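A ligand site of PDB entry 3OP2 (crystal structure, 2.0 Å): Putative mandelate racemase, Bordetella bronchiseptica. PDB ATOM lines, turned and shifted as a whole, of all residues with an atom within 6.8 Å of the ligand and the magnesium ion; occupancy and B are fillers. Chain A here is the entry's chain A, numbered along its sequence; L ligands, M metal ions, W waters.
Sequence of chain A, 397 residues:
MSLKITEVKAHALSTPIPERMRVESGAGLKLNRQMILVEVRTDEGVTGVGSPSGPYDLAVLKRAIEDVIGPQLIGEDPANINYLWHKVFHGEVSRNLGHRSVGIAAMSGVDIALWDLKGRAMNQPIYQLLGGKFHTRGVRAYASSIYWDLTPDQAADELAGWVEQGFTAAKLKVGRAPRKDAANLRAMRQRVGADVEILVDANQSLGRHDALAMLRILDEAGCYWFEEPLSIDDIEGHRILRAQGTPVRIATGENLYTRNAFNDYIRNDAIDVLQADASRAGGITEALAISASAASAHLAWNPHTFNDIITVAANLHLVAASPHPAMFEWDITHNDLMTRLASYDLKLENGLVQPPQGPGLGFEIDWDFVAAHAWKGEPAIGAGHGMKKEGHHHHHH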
ATOM      1  N   GLU A  24       2.601  -5.856  -6.479  1.00  0.00           N
ATOM      2  CA  GLU A  24       1.477  -6.668  -5.994  1.00  0.00           C
ATOM      3  C   GLU A  24       0.305  -5.833  -5.424  1.00  0.00           C
ATOM      4  O   GLU A  24      -0.855  -6.135  -5.692  1.00  0.00           O
ATOM      5  CB  GLU A  24       1.960  -7.734  -5.001  1.00  0.00           C
ATOM      6  CG  GLU A  24       2.933  -8.740  -5.648  1.00  0.00           C
ATOM      7  CD  GLU A  24       3.327  -9.912  -4.748  1.00  0.00           C
ATOM      8  OE1 GLU A  24       3.480  -9.714  -3.521  1.00  0.00           O
ATOM      9  OE2 GLU A  24       3.485 -11.037  -5.272  1.00  0.00           O
ATOM     10  N   LYS A  30       7.522  -2.189 -11.031  1.00  0.00           N
ATOM     11  CA  LYS A  30       8.801  -2.847 -10.792  1.00  0.00           C
ATOM     12  C   LYS A  30       9.774  -2.394 -11.874  1.00  0.00           C
ATOM     13  O   LYS A  30       9.662  -2.782 -13.034  1.00  0.00           O
ATOM     14  CB  LYS A  30       8.613  -4.358 -10.837  1.00  0.00           C
ATOM     15  CG  LYS A  30       7.741  -4.920  -9.748  1.00  0.00           C
ATOM     16  CD  LYS A  30       7.112  -6.226 -10.204  1.00  0.00           C
ATOM     17  CE  LYS A  30       6.345  -6.902  -9.071  1.00  0.00           C
ATOM     18  NZ  LYS A  30       5.494  -8.046  -9.546  1.00  0.00           N
ATOM     19  N   ARG A  33      15.918  -4.705 -11.595  1.00  0.00           N
ATOM     20  CA  ARG A  33      16.442  -5.768 -10.741  1.00  0.00           C
ATOM     21  C   ARG A  33      17.772  -5.277 -10.194  1.00  0.00           C
ATOM     22  O   ARG A  33      18.606  -4.734 -10.942  1.00  0.00           O
ATOM     23  CB  ARG A  33      16.615  -7.066 -11.525  1.00  0.00           C
ATOM     24  CG  ARG A  33      15.418  -7.399 -12.387  1.00  0.00           C
ATOM     25  CD  ARG A  33      15.309  -8.864 -12.721  1.00  0.00           C
ATOM     26  NE  ARG A  33      14.792  -9.659 -11.607  1.00  0.00           N
ATOM     27  CZ  ARG A  33      13.494  -9.893 -11.390  1.00  0.00           C
ATOM     28  NH1 ARG A  33      12.568  -9.397 -12.203  1.00  0.00           N
ATOM     29  NH2 ARG A  33      13.122 -10.630 -10.344  1.00  0.00           N
ATOM     30  N   TYR A 142      12.196 -26.817  -7.834  1.00  0.00           N
ATOM     31  CA  TYR A 142      10.837 -26.396  -8.158  1.00  0.00           C
ATOM     32  C   TYR A 142      10.823 -25.048  -8.877  1.00  0.00           C
ATOM     33  O   TYR A 142      11.730 -24.214  -8.666  1.00  0.00           O
ATOM     34  CB  TYR A 142       9.903 -26.439  -6.934  1.00  0.00           C
ATOM     35  CG  TYR A 142      10.094 -25.355  -5.911  1.00  0.00           C
ATOM     36  CD1 TYR A 142       9.404 -24.146  -6.018  1.00  0.00           C
ATOM     37  CD2 TYR A 142      10.939 -25.534  -4.815  1.00  0.00           C
ATOM     38  CE1 TYR A 142       9.561 -23.132  -5.077  1.00  0.00           C
ATOM     39  CE2 TYR A 142      11.102 -24.527  -3.852  1.00  0.00           C
ATOM     40  CZ  TYR A 142      10.398 -23.336  -3.995  1.00  0.00           C
ATOM     41  OH  TYR A 142      10.554 -22.314  -3.069  1.00  0.00           O
ATOM     42  N   SER A 144       9.573 -21.421  -9.444  1.00  0.00           N
ATOM     43  CA  SER A 144       9.001 -20.349  -8.625  1.00  0.00           C
ATOM     44  C   SER A 144       8.899 -19.017  -9.387  1.00  0.00           C
ATOM     45  O   SER A 144       9.917 -18.464  -9.823  1.00  0.00           O
ATOM     46  CB  SER A 144       9.839 -20.147  -7.367  1.00  0.00           C
ATOM     47  OG  SER A 144       9.328 -19.075  -6.583  1.00  0.00           O
ATOM     48  N   SER A 145       7.688 -18.479  -9.550  1.00  0.00           N
ATOM     49  CA  SER A 145       6.447 -19.067  -9.042  1.00  0.00           C
ATOM     50  C   SER A 145       5.285 -18.650  -9.945  1.00  0.00           C
ATOM     51  O   SER A 145       5.394 -17.692 -10.705  1.00  0.00           O
ATOM     52  CB  SER A 145       6.160 -18.615  -7.595  1.00  0.00           C
ATOM     53  OG  SER A 145       6.286 -17.211  -7.453  1.00  0.00           O
ATOM     54  N   TYR A 147       1.875 -16.901 -10.536  1.00  0.00           N
ATOM     55  CA  TYR A 147       1.122 -15.780  -9.970  1.00  0.00           C
ATOM     56  C   TYR A 147      -0.320 -16.187  -9.622  1.00  0.00           C
ATOM     57  O   TYR A 147      -0.900 -17.069 -10.264  1.00  0.00           O
ATOM     58  CB  TYR A 147       1.122 -14.606 -10.949  1.00  0.00           C
ATOM     59  CG  TYR A 147       0.835 -13.270 -10.309  1.00  0.00           C
ATOM     60  CD1 TYR A 147       1.732 -12.685  -9.418  1.00  0.00           C
ATOM     61  CD2 TYR A 147      -0.337 -12.575 -10.619  1.00  0.00           C
ATOM     62  CE1 TYR A 147       1.482 -11.442  -8.845  1.00  0.00           C
ATOM     63  CE2 TYR A 147      -0.602 -11.335 -10.047  1.00  0.00           C
ATOM     64  CZ  TYR A 147       0.304 -10.781  -9.166  1.00  0.00           C
ATOM     65  OH  TYR A 147       0.041  -9.542  -8.607  1.00  0.00           O
ATOM     66  N   LYS A 171       5.631 -23.881  -7.512  1.00  0.00           N
ATOM     67  CA  LYS A 171       4.974 -23.108  -6.436  1.00  0.00           C
ATOM     68  C   LYS A 171       3.959 -22.093  -6.974  1.00  0.00           C
ATOM     69  O   LYS A 171       4.247 -21.344  -7.931  1.00  0.00           O
ATOM     70  CB  LYS A 171       6.022 -22.418  -5.568  1.00  0.00           C
ATOM     71  CG  LYS A 171       5.500 -21.793  -4.278  1.00  0.00           C
ATOM     72  CD  LYS A 171       6.653 -21.552  -3.311  1.00  0.00           C
ATOM     73  CE  LYS A 171       7.400 -20.275  -3.654  1.00  0.00           C
ATOM     74  NZ  LYS A 171       8.626 -20.075  -2.825  1.00  0.00           N
ATOM     75  N   LYS A 173       1.382 -18.845  -5.934  1.00  0.00           N
ATOM     76  CA  LYS A 173       0.966 -17.786  -5.025  1.00  0.00           C
ATOM     77  C   LYS A 173      -0.520 -17.910  -4.732  1.00  0.00           C
ATOM     78  O   LYS A 173      -1.319 -18.182  -5.628  1.00  0.00           O
ATOM     79  CB  LYS A 173       1.310 -16.404  -5.579  1.00  0.00           C
ATOM     80  CG  LYS A 173       2.773 -16.030  -5.392  1.00  0.00           C
ATOM     81  CD  LYS A 173       3.104 -14.668  -5.996  1.00  0.00           C
ATOM     82  CE  LYS A 173       4.441 -14.152  -5.515  1.00  0.00           C
ATOM     83  NZ  LYS A 173       5.558 -15.092  -5.823  1.00  0.00           N
ATOM     84  N   ASP A 201       2.351 -20.491  -1.689  1.00  0.00           N
ATOM     85  CA  ASP A 201       3.008 -19.401  -0.937  1.00  0.00           C
ATOM     86  C   ASP A 201       1.996 -18.278  -0.692  1.00  0.00           C
ATOM     87  O   ASP A 201       1.471 -17.694  -1.656  1.00  0.00           O
ATOM     88  CB  ASP A 201       4.240 -18.859  -1.713  1.00  0.00           C
ATOM     89  CG  ASP A 201       5.127 -17.922  -0.886  1.00  0.00           C
ATOM     90  OD1 ASP A 201       4.665 -17.242   0.062  1.00  0.00           O
ATOM     91  OD2 ASP A 201       6.334 -17.838  -1.220  1.00  0.00           O
ATOM     92  N   ALA A 202       1.720 -17.981   0.571  1.00  0.00           N
ATOM     93  CA  ALA A 202       0.687 -16.977   0.897  1.00  0.00           C
ATOM     94  C   ALA A 202       1.268 -15.592   1.169  1.00  0.00           C
ATOM     95  O   ALA A 202       0.532 -14.624   1.294  1.00  0.00           O
ATOM     96  CB  ALA A 202      -0.188 -17.437   2.061  1.00  0.00           C
ATOM     97  N   ASN A 203       2.586 -15.512   1.261  1.00  0.00           N
ATOM     98  CA  ASN A 203       3.298 -14.257   1.481  1.00  0.00           C
ATOM     99  C   ASN A 203       2.783 -13.485   2.694  1.00  0.00           C
ATOM    100  O   ASN A 203       2.671 -12.265   2.648  1.00  0.00           O
ATOM    101  CB  ASN A 203       3.308 -13.398   0.198  1.00  0.00           C
ATOM    102  CG  ASN A 203       4.105 -14.039  -0.925  1.00  0.00           C
ATOM    103  OD1 ASN A 203       3.538 -14.612  -1.860  1.00  0.00           O
ATOM    104  ND2 ASN A 203       5.426 -13.977  -0.815  1.00  0.00           N
ATOM    105  N   GLU A 227       3.559 -22.093   2.443  1.00  0.00           N
ATOM    106  CA  GLU A 227       4.662 -21.161   2.730  1.00  0.00           C
ATOM    107  C   GLU A 227       4.156 -19.796   3.192  1.00  0.00           C
ATOM    108  O   GLU A 227       3.164 -19.273   2.648  1.00  0.00           O
ATOM    109  CB  GLU A 227       5.574 -21.023   1.480  1.00  0.00           C
ATOM    110  CG  GLU A 227       6.764 -20.045   1.628  1.00  0.00           C
ATOM    111  CD  GLU A 227       7.754 -20.097   0.455  1.00  0.00           C
ATOM    112  OE1 GLU A 227       7.797 -21.100  -0.279  1.00  0.00           O
ATOM    113  OE2 GLU A 227       8.520 -19.126   0.286  1.00  0.00           O
ATOM    114  N   GLU A 228       4.830 -19.231   4.190  1.00  0.00           N
ATOM    115  CA  GLU A 228       4.397 -17.991   4.844  1.00  0.00           C
ATOM    116  C   GLU A 228       2.864 -17.853   4.921  1.00  0.00           C
ATOM    117  O   GLU A 228       2.272 -16.928   4.338  1.00  0.00           O
ATOM    118  CB  GLU A 228       5.031 -16.761   4.172  1.00  0.00           C
ATOM    119  CG  GLU A 228       6.566 -16.686   4.303  1.00  0.00           C
ATOM    120  CD  GLU A 228       7.103 -15.288   4.011  1.00  0.00           C
ATOM    121  OE1 GLU A 228       6.778 -14.711   2.940  1.00  0.00           O
ATOM    122  OE2 GLU A 228       7.864 -14.754   4.842  1.00  0.00           O
ATOM    123  N   GLU A 254      12.091 -17.075   4.656  1.00  0.00           N
ATOM    124  CA  GLU A 254      12.801 -16.119   3.797  1.00  0.00           C
ATOM    125  C   GLU A 254      12.973 -14.745   4.440  1.00  0.00           C
ATOM    126  O   GLU A 254      13.896 -13.996   4.096  1.00  0.00           O
ATOM    127  CB  GLU A 254      12.124 -15.994   2.439  1.00  0.00           C
ATOM    128  CG  GLU A 254      10.793 -15.291   2.505  1.00  0.00           C
ATOM    129  CD  GLU A 254      10.027 -15.364   1.228  1.00  0.00           C
ATOM    130  OE1 GLU A 254       9.927 -14.331   0.559  1.00  0.00           O
ATOM    131  OE2 GLU A 254       9.509 -16.452   0.892  1.00  0.00           O
ATOM    132  N   ASN A 255      12.074 -14.421   5.375  1.00  0.00           N
ATOM    133  CA  ASN A 255      12.090 -13.149   6.082  1.00  0.00           C
ATOM    134  C   ASN A 255      12.560 -13.239   7.543  1.00  0.00           C
ATOM    135  O   ASN A 255      12.415 -12.279   8.305  1.00  0.00           O
ATOM    136  CB  ASN A 255      10.710 -12.488   5.989  1.00  0.00           C
ATOM    137  CG  ASN A 255      10.381 -12.015   4.585  1.00  0.00           C
ATOM    138  OD1 ASN A 255       9.300 -12.310   4.053  1.00  0.00           O
ATOM    139  ND2 ASN A 255      11.294 -11.280   3.977  1.00  0.00           N
ATOM    140  N   GLN A 275      13.218 -22.101   5.804  1.00  0.00           N
ATOM    141  CA  GLN A 275      13.562 -21.569   4.489  1.00  0.00           C
ATOM    142  C   GLN A 275      14.563 -20.428   4.565  1.00  0.00           C
ATOM    143  O   GLN A 275      14.618 -19.584   3.660  1.00  0.00           O
ATOM    144  CB  GLN A 275      12.300 -21.112   3.771  1.00  0.00           C
ATOM    145  CG  GLN A 275      11.302 -22.233   3.514  1.00  0.00           C
ATOM    146  CD  GLN A 275      10.058 -21.760   2.804  1.00  0.00           C
ATOM    147  OE1 GLN A 275       9.295 -20.975   3.352  1.00  0.00           O
ATOM    148  NE2 GLN A 275       9.843 -22.242   1.584  1.00  0.00           N
ATOM    149  N   HIS A 304      14.978 -20.409   0.807  1.00  0.00           N
ATOM    150  CA  HIS A 304      14.634 -19.402  -0.186  1.00  0.00           C
ATOM    151  C   HIS A 304      15.945 -19.005  -0.861  1.00  0.00           C
ATOM    152  O   HIS A 304      16.942 -18.813  -0.163  1.00  0.00           O
ATOM    153  CB  HIS A 304      14.041 -18.213   0.534  1.00  0.00           C
ATOM    154  CG  HIS A 304      13.862 -17.005  -0.325  1.00  0.00           C
ATOM    155  ND1 HIS A 304      14.874 -16.096  -0.553  1.00  0.00           N
ATOM    156  CD2 HIS A 304      12.778 -16.541  -1.002  1.00  0.00           C
ATOM    157  CE1 HIS A 304      14.427 -15.129  -1.332  1.00  0.00           C
ATOM    158  NE2 HIS A 304      13.159 -15.375  -1.610  1.00  0.00           N
ATOM    159  N   THR A 305      15.951 -18.877  -2.187  1.00  0.00           N
ATOM    160  CA  THR A 305      17.197 -18.630  -2.948  1.00  0.00           C
ATOM    161  C   THR A 305      17.138 -17.389  -3.861  1.00  0.00           C
ATOM    162  O   THR A 305      18.141 -16.984  -4.463  1.00  0.00           O
ATOM    163  CB  THR A 305      17.585 -19.848  -3.837  1.00  0.00           C
ATOM    164  OG1 THR A 305      16.686 -19.942  -4.948  1.00  0.00           O
ATOM    165  CG2 THR A 305      17.563 -21.164  -3.047  1.00  0.00           C
ATOM    166  N   PHE A 306      15.950 -16.794  -3.941  1.00  0.00           N
ATOM    167  CA  PHE A 306      15.497 -15.846  -4.947  1.00  0.00           C
ATOM    168  C   PHE A 306      16.167 -14.463  -4.866  1.00  0.00           C
ATOM    169  O   PHE A 306      15.834 -13.667  -3.979  1.00  0.00           O
ATOM    170  CB  PHE A 306      13.979 -15.706  -4.711  1.00  0.00           C
ATOM    171  CG  PHE A 306      13.192 -15.102  -5.842  1.00  0.00           C
ATOM    172  CD1 PHE A 306      13.278 -13.741  -6.144  1.00  0.00           C
ATOM    173  CD2 PHE A 306      12.279 -15.887  -6.565  1.00  0.00           C
ATOM    174  CE1 PHE A 306      12.507 -13.183  -7.168  1.00  0.00           C
ATOM    175  CE2 PHE A 306      11.507 -15.342  -7.610  1.00  0.00           C
ATOM    176  CZ  PHE A 306      11.613 -13.975  -7.903  1.00  0.00           C
ATOM    177  N   GLU A 329      14.328 -23.995  -4.653  1.00  0.00           N
ATOM    178  CA  GLU A 329      13.681 -22.901  -5.352  1.00  0.00           C
ATOM    179  C   GLU A 329      14.477 -22.434  -6.561  1.00  0.00           C
ATOM    180  O   GLU A 329      15.640 -22.013  -6.425  1.00  0.00           O
ATOM    181  CB  GLU A 329      13.445 -21.731  -4.398  1.00  0.00           C
ATOM    182  CG  GLU A 329      12.748 -20.562  -5.066  1.00  0.00           C
ATOM    183  CD  GLU A 329      12.348 -19.464  -4.116  1.00  0.00           C
ATOM    184  OE1 GLU A 329      13.123 -19.162  -3.182  1.00  0.00           O
ATOM    185  OE2 GLU A 329      11.258 -18.901  -4.318  1.00  0.00           O
ATOM    186  N   THR A 333      11.469 -16.388 -13.322  1.00  0.00           N
ATOM    187  CA  THR A 333      11.170 -15.100 -13.966  1.00  0.00           C
ATOM    188  C   THR A 333      12.365 -14.579 -14.758  1.00  0.00           C
ATOM    189  O   THR A 333      13.517 -14.966 -14.517  1.00  0.00           O
ATOM    190  CB  THR A 333      10.728 -14.002 -12.942  1.00  0.00           C
ATOM    191  OG1 THR A 333      11.848 -13.565 -12.169  1.00  0.00           O
ATOM    192  CG2 THR A 333       9.616 -14.510 -12.034  1.00  0.00           C
HETATM  193  C1  LIG L   1       9.530 -16.449  -2.822  1.00  0.00           C
HETATM  194  O1  LIG L   1      10.453 -16.466  -3.664  1.00  0.00           O
HETATM  195  O2  LIG L   1       9.319 -17.419  -2.044  1.00  0.00           O
HETATM  196  C2  LIG L   1       8.688 -15.268  -2.693  1.00  0.00           C
HETATM  197  O3  LIG L   1       7.817 -15.267  -1.823  1.00  0.00           O
HETATM  198  C3  LIG L   1       8.875 -14.034  -3.550  1.00  0.00           C
HETATM  199  C4  LIG L   1       8.612 -14.322  -5.030  1.00  0.00           C
HETATM  200  C5  LIG L   1       8.231 -13.069  -5.808  1.00  0.00           C
HETATM  201  O4  LIG L   1       8.847 -11.997  -5.624  1.00  0.00           O
HETATM  202  O5  LIG L   1       7.315 -13.156  -6.657  1.00  0.00           O
HETATM  203 MG    MG M   1       8.143 -17.165  -0.295  1.00  0.00          MG
HETATM  204  O   HOH W   1       6.806 -16.276   1.116  1.00  0.00           O
HETATM  205  O   HOH W   2      11.866 -12.879  -2.287  1.00  0.00           O
HETATM  206  O   HOH W   3      11.088 -19.583  -0.533  1.00  0.00           O
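O1 of the ligand sits close to OE2 of Glu 329, at 2.6 Å. NZ of Lys 173 is in salt-bridge range of O5 of the ligand, 2.7 Å away. The side-chain amino group (NZ) of Lys 171 sits close to an oxygen (O2) of the ligand (2.9 Å). O3 of the ligand sits close to ND2 of Asn 203 (2.9 Å).
The side-chain carboxylate (OE1) of Glu 227 lies within hydrogen-bond range of the side-chain amide nitrogen (NE2) of Gln 275, 3.0 Å away. O of Glu 227 sits at hydrogen-bond distance from N of Ala 202 (2.8 Å). The side-chain carboxylate of Glu 329 lies within salt-bridge range of the side-chain amino group of Lys 171. The side-chain carboxylate (OE2) of Glu 329 lies within hydrogen-bond range of the side-chain hydroxyl (OG) of Ser 144 (3.0 Å). O of Glu 329 sits at hydrogen-bond distance from OG1 of Thr 305, 2.8 Å away. The side-chain hydroxyl (OG) of Ser 145 sits at hydrogen-bond distance from the side-chain amino group (NZ) of Lys 173 (2.8 Å). The side-chain amino group (NZ) of Lys 171 is in hydrogen-bond range of the side-chain hydroxyl (OH) of Tyr 142, 3.0 Å away. The backbone carbonyl oxygen (O) of Gln 275 is in hydrogen-bond range of the backbone NH (N) of His 304, at 3.0 Å.
Merely in contact with the ligand: His 304 and Phe 306. Hydrophobic or aromatic side chains that line the ligand: His 304 and Phe 306. Within 4 Å of the ligand: Lys 171, Lys 173, Asp 201, Asn 203, Glu 227, Glu 254, His 304, Phe 306 and Glu 329.
Residues that only touch the magnesium ion: Lys 171. The nearest printed residue that does not touch the magnesium ion is Asn 203 (4.2 Å).
The magnesium ion is bound by OE2 of Glu 254 (1.9 Å). The magnesium ion is bound by OE2 of Glu 227 (2.1 Å). The magnesium ion is bound by an oxygen (O2) of the ligand (2.1 Å). Water W1 is bound to the magnesium ion (2.1 Å). The magnesium ion is bound by OD2 of Asp 201. O3 of the ligand binds the magnesium ion, 2.5 Å away.
Water W1 lies within hydrogen-bond range of the side-chain carboxylate (OE1) of Glu 228 (2.4 Å), the side-chain carboxylate (OD1) of Asp 201 (2.6 Å) and the side-chain amide nitrogen (ND2) of Asn 203 (3.3 Å). Water W3 lies within hydrogen-bond range of OE1 of Glu 329 and NZ of Lys 171.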
